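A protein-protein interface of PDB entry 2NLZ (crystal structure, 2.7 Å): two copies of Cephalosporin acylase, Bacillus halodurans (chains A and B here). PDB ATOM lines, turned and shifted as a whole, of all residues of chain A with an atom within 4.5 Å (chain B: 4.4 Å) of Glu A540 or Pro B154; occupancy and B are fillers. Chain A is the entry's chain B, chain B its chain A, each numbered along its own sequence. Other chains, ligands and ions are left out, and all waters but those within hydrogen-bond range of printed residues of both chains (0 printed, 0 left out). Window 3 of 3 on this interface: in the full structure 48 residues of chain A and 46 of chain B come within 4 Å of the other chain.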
ATOM      1  N   TYR A  20     -12.127  -6.882  -3.771  1.00  0.00           N
ATOM      2  CA  TYR A  20     -11.348  -6.248  -4.819  1.00  0.00           C
ATOM      3  C   TYR A  20      -9.943  -6.814  -4.916  1.00  0.00           C
ATOM      4  O   TYR A  20      -9.328  -7.143  -3.905  1.00  0.00           O
ATOM      5  CB  TYR A  20     -11.298  -4.739  -4.605  1.00  0.00           C
ATOM      6  CG  TYR A  20     -12.575  -4.035  -4.985  1.00  0.00           C
ATOM      7  CD1 TYR A  20     -12.690  -3.400  -6.217  1.00  0.00           C
ATOM      8  CD2 TYR A  20     -13.672  -4.014  -4.120  1.00  0.00           C
ATOM      9  CE1 TYR A  20     -13.861  -2.754  -6.585  1.00  0.00           C
ATOM     10  CE2 TYR A  20     -14.849  -3.379  -4.480  1.00  0.00           C
ATOM     11  CZ  TYR A  20     -14.936  -2.747  -5.711  1.00  0.00           C
ATOM     12  OH  TYR A  20     -16.092  -2.102  -6.070  1.00  0.00           O
ATOM     13  N   ALA A  21      -9.450  -6.937  -6.148  1.00  0.00           N
ATOM     14  CA  ALA A  21      -8.065  -7.332  -6.410  1.00  0.00           C
ATOM     15  C   ALA A  21      -7.501  -6.702  -7.688  1.00  0.00           C
ATOM     16  O   ALA A  21      -8.231  -6.082  -8.458  1.00  0.00           O
ATOM     17  CB  ALA A  21      -7.956  -8.831  -6.481  1.00  0.00           C
ATOM     18  N   LYS A  22      -6.198  -6.862  -7.897  1.00  0.00           N
ATOM     19  CA  LYS A  22      -5.537  -6.423  -9.124  1.00  0.00           C
ATOM     20  C   LYS A  22      -4.805  -7.576  -9.805  1.00  0.00           C
ATOM     21  O   LYS A  22      -4.961  -7.803 -11.011  1.00  0.00           O
ATOM     22  CB  LYS A  22      -4.550  -5.284  -8.836  1.00  0.00           C
ATOM     23  CG  LYS A  22      -5.145  -3.878  -8.884  1.00  0.00           C
ATOM     24  CD  LYS A  22      -5.516  -3.446 -10.309  1.00  0.00           C
ATOM     25  CE  LYS A  22      -4.289  -3.175 -11.192  1.00  0.00           C
ATOM     26  NZ  LYS A  22      -3.623  -1.885 -10.874  1.00  0.00           N
ATOM     27  N   ASN A  23      -4.014  -8.307  -9.026  1.00  0.00           N
ATOM     28  CA  ASN A  23      -3.089  -9.289  -9.588  1.00  0.00           C
ATOM     29  C   ASN A  23      -3.655 -10.692  -9.692  1.00  0.00           C
ATOM     30  O   ASN A  23      -3.053 -11.564 -10.325  1.00  0.00           O
ATOM     31  CB  ASN A  23      -1.744  -9.293  -8.839  1.00  0.00           C
ATOM     32  CG  ASN A  23      -0.889  -8.067  -9.156  1.00  0.00           C
ATOM     33  OD1 ASN A  23      -0.041  -7.671  -8.359  1.00  0.00           O
ATOM     34  ND2 ASN A  23      -1.113  -7.462 -10.322  1.00  0.00           N
ATOM     35  N   ALA A 538      -8.463 -12.641  -2.930  1.00  0.00           N
ATOM     36  CA  ALA A 538      -7.537 -11.799  -3.684  1.00  0.00           C
ATOM     37  C   ALA A 538      -6.090 -12.292  -3.562  1.00  0.00           C
ATOM     38  O   ALA A 538      -5.711 -12.899  -2.553  1.00  0.00           O
ATOM     39  CB  ALA A 538      -7.644 -10.357  -3.204  1.00  0.00           C
ATOM     40  N   TRP A 539      -5.293 -12.042  -4.597  1.00  0.00           N
ATOM     41  CA  TRP A 539      -3.852 -12.254  -4.522  1.00  0.00           C
ATOM     42  C   TRP A 539      -3.121 -11.042  -5.080  1.00  0.00           C
ATOM     43  O   TRP A 539      -3.484 -10.548  -6.160  1.00  0.00           O
ATOM     44  CB  TRP A 539      -3.437 -13.510  -5.283  1.00  0.00           C
ATOM     45  CG  TRP A 539      -1.945 -13.658  -5.390  1.00  0.00           C
ATOM     46  CD1 TRP A 539      -1.070 -13.921  -4.374  1.00  0.00           C
ATOM     47  CD2 TRP A 539      -1.154 -13.531  -6.576  1.00  0.00           C
ATOM     48  NE1 TRP A 539       0.215 -13.971  -4.855  1.00  0.00           N
ATOM     49  CE2 TRP A 539       0.192 -13.736  -6.204  1.00  0.00           C
ATOM     50  CE3 TRP A 539      -1.452 -13.266  -7.920  1.00  0.00           C
ATOM     51  CZ2 TRP A 539       1.240 -13.694  -7.128  1.00  0.00           C
ATOM     52  CZ3 TRP A 539      -0.407 -13.218  -8.840  1.00  0.00           C
ATOM     53  CH2 TRP A 539       0.922 -13.430  -8.437  1.00  0.00           C
ATOM     54  N   GLU A 540      -2.100 -10.562  -4.355  1.00  0.00           N
ATOM     55  CA  GLU A 540      -1.363  -9.360  -4.781  1.00  0.00           C
ATOM     56  C   GLU A 540       0.177  -9.443  -4.851  1.00  0.00           C
ATOM     57  O   GLU A 540       0.847  -8.416  -4.713  1.00  0.00           O
ATOM     58  CB  GLU A 540      -1.774  -8.155  -3.944  1.00  0.00           C
ATOM     59  CG  GLU A 540      -3.272  -7.907  -3.868  1.00  0.00           C
ATOM     60  CD  GLU A 540      -3.907  -7.520  -5.197  1.00  0.00           C
ATOM     61  OE1 GLU A 540      -3.183  -7.204  -6.185  1.00  0.00           O
ATOM     62  OE2 GLU A 540      -5.155  -7.513  -5.229  1.00  0.00           O
ATOM     63  N   GLY A 541       0.727 -10.643  -5.090  1.00  0.00           N
ATOM     64  CA  GLY A 541       2.180 -10.832  -5.302  1.00  0.00           C
ATOM     65  C   GLY A 541       2.633 -10.605  -6.743  1.00  0.00           C
ATOM     66  O   GLY A 541       1.933  -9.939  -7.521  1.00  0.00           O
ATOM     67  N   LEU B  32      -6.254  -9.774   3.123  1.00  0.00           N
ATOM     68  CA  LEU B  32      -4.855 -10.048   2.855  1.00  0.00           C
ATOM     69  C   LEU B  32      -4.033 -10.153   4.152  1.00  0.00           C
ATOM     70  O   LEU B  32      -2.982 -10.799   4.186  1.00  0.00           O
ATOM     71  CB  LEU B  32      -4.280  -8.977   1.933  1.00  0.00           C
ATOM     72  CG  LEU B  32      -4.942  -8.812   0.561  1.00  0.00           C
ATOM     73  CD1 LEU B  32      -4.582  -7.456  -0.049  1.00  0.00           C
ATOM     74  CD2 LEU B  32      -4.565  -9.981  -0.368  1.00  0.00           C
ATOM     75  N   GLU B 151       5.556  -3.741  -2.573  1.00  0.00           N
ATOM     76  CA  GLU B 151       4.860  -3.982  -3.832  1.00  0.00           C
ATOM     77  C   GLU B 151       3.565  -3.190  -3.938  1.00  0.00           C
ATOM     78  O   GLU B 151       3.190  -2.756  -5.024  1.00  0.00           O
ATOM     79  CB  GLU B 151       4.624  -5.484  -4.040  1.00  0.00           C
ATOM     80  CG  GLU B 151       5.915  -6.251  -4.379  1.00  0.00           C
ATOM     81  CD  GLU B 151       5.817  -7.760  -4.165  1.00  0.00           C
ATOM     82  OE1 GLU B 151       6.882  -8.387  -3.966  1.00  0.00           O
ATOM     83  OE2 GLU B 151       4.695  -8.320  -4.194  1.00  0.00           O
ATOM     84  N   TYR B 153      -0.751  -2.423  -2.626  1.00  0.00           N
ATOM     85  CA  TYR B 153      -2.045  -3.099  -2.671  1.00  0.00           C
ATOM     86  C   TYR B 153      -3.142  -2.161  -3.173  1.00  0.00           C
ATOM     87  O   TYR B 153      -3.059  -0.946  -2.967  1.00  0.00           O
ATOM     88  CB  TYR B 153      -2.414  -3.677  -1.293  1.00  0.00           C
ATOM     89  CG  TYR B 153      -2.557  -2.647  -0.199  1.00  0.00           C
ATOM     90  CD1 TYR B 153      -3.797  -2.104   0.115  1.00  0.00           C
ATOM     91  CD2 TYR B 153      -1.447  -2.225   0.533  1.00  0.00           C
ATOM     92  CE1 TYR B 153      -3.925  -1.154   1.119  1.00  0.00           C
ATOM     93  CE2 TYR B 153      -1.566  -1.284   1.539  1.00  0.00           C
ATOM     94  CZ  TYR B 153      -2.802  -0.751   1.825  1.00  0.00           C
ATOM     95  OH  TYR B 153      -2.908   0.190   2.823  1.00  0.00           O
ATOM     96  N   PRO B 154      -4.166  -2.720  -3.852  1.00  0.00           N
ATOM     97  CA  PRO B 154      -5.321  -1.931  -4.252  1.00  0.00           C
ATOM     98  C   PRO B 154      -6.215  -1.578  -3.068  1.00  0.00           C
ATOM     99  O   PRO B 154      -6.431  -2.392  -2.168  1.00  0.00           O
ATOM    100  CB  PRO B 154      -6.050  -2.846  -5.230  1.00  0.00           C
ATOM    101  CG  PRO B 154      -5.632  -4.213  -4.866  1.00  0.00           C
ATOM    102  CD  PRO B 154      -4.265  -4.120  -4.306  1.00  0.00           C
ATOM    103  N   VAL B 155      -6.721  -0.355  -3.080  1.00  0.00           N
ATOM    104  CA  VAL B 155      -7.494   0.169  -1.967  1.00  0.00           C
ATOM    105  C   VAL B 155      -8.982  -0.134  -2.151  1.00  0.00           C
ATOM    106  O   VAL B 155      -9.583   0.219  -3.162  1.00  0.00           O
ATOM    107  CB  VAL B 155      -7.242   1.690  -1.791  1.00  0.00           C
ATOM    108  CG1 VAL B 155      -8.154   2.287  -0.721  1.00  0.00           C
ATOM    109  CG2 VAL B 155      -5.772   1.948  -1.458  1.00  0.00           C
ATOM    110  N   THR B 156      -9.559  -0.804  -1.163  1.00  0.00           N
ATOM    111  CA  THR B 156     -10.975  -1.140  -1.173  1.00  0.00           C
ATOM    112  C   THR B 156     -11.816   0.097  -0.844  1.00  0.00           C
ATOM    113  O   THR B 156     -11.320   1.013  -0.192  1.00  0.00           O
ATOM    114  CB  THR B 156     -11.271  -2.281  -0.175  1.00  0.00           C
ATOM    115  OG1 THR B 156     -11.196  -1.782   1.168  1.00  0.00           O
ATOM    116  CG2 THR B 156     -10.274  -3.435  -0.382  1.00  0.00           C
ATOM    117  N   GLY B 196      -9.383   1.133  -5.961  1.00  0.00           N
ATOM    118  CA  GLY B 196      -8.653   0.374  -6.968  1.00  0.00           C
ATOM    119  C   GLY B 196      -7.256   0.896  -7.242  1.00  0.00           C
ATOM    120  O   GLY B 196      -6.458   0.235  -7.920  1.00  0.00           O
ATOM    121  N   GLU B 197      -6.960   2.085  -6.731  1.00  0.00           N
ATOM    122  CA  GLU B 197      -5.635   2.670  -6.870  1.00  0.00           C
ATOM    123  C   GLU B 197      -4.665   1.916  -5.961  1.00  0.00           C
ATOM    124  O   GLU B 197      -5.029   1.530  -4.849  1.00  0.00           O
ATOM    125  CB  GLU B 197      -5.685   4.160  -6.516  1.00  0.00           C
ATOM    126  CG  GLU B 197      -4.482   4.989  -6.979  1.00  0.00           C
ATOM    127  CD  GLU B 197      -4.550   6.440  -6.504  1.00  0.00           C
ATOM    128  OE1 GLU B 197      -3.485   7.098  -6.430  1.00  0.00           O
ATOM    129  OE2 GLU B 197      -5.669   6.923  -6.203  1.00  0.00           O
ATOM    130  N   VAL B 198      -3.449   1.680  -6.441  1.00  0.00           N
ATOM    131  CA  VAL B 198      -2.449   0.985  -5.636  1.00  0.00           C
ATOM    132  C   VAL B 198      -1.706   1.996  -4.780  1.00  0.00           C
ATOM    133  O   VAL B 198      -1.309   3.055  -5.275  1.00  0.00           O
ATOM    134  CB  VAL B 198      -1.463   0.182  -6.507  1.00  0.00           C
ATOM    135  CG1 VAL B 198      -0.197  -0.166  -5.735  1.00  0.00           C
ATOM    136  CG2 VAL B 198      -2.128  -1.077  -7.014  1.00  0.00           C
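Among the printed residues, pairs that only touch across the chains: Lys A22 with Pro B154 (3.9 Å), Ala A538 with Leu B32 (3.8 Å), Glu A540 with Glu B151 (3.9 Å), Glu A540 with Pro B154 (3.4 Å) and Gly A541 with Glu B151 (3.7 Å).
N of Asn A23 lies within hydrogen-bond range of OE1 of Glu A540, 3.2 Å away. The side-chain amide oxygen of Asn A23 sits close to the backbone carbonyl oxygen of Gly A541, at 3.1 Å. The backbone NH (N) of Lys A22 sits at hydrogen-bond distance from the side-chain carboxylate (OE2) of Glu A540, 2.9 Å away.
Of the printed residues of chain B, Lys A22 touches Pro B154. Of the printed residues of chain B, Ala A538 touches Leu B32 (3.8 Å). Printed residues of chain B within 4 Å of Glu A540: Glu B151 (3.9 Å) and Pro B154 (3.4 Å). Of the printed residues of chain B, Gly A541 touches Glu B151. Of the printed residues of chain A, Leu B32 touches Ala A538 (3.8 Å). Of the printed residues of chain A, Glu B151 touches Glu A540 and Gly A541. Of the printed residues of chain A, Pro B154 touches Lys A22 and Glu A540.
Printed residues of chain A that touch a printed residue of chain B: Lys A22, Ala A538, Glu A540 and Gly A541. Among the printed residues, no Asp or Glu carboxylate lies within 4 Å of a Lys or Arg side-chain nitrogen of the other chain.
No position is printed for both chains.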
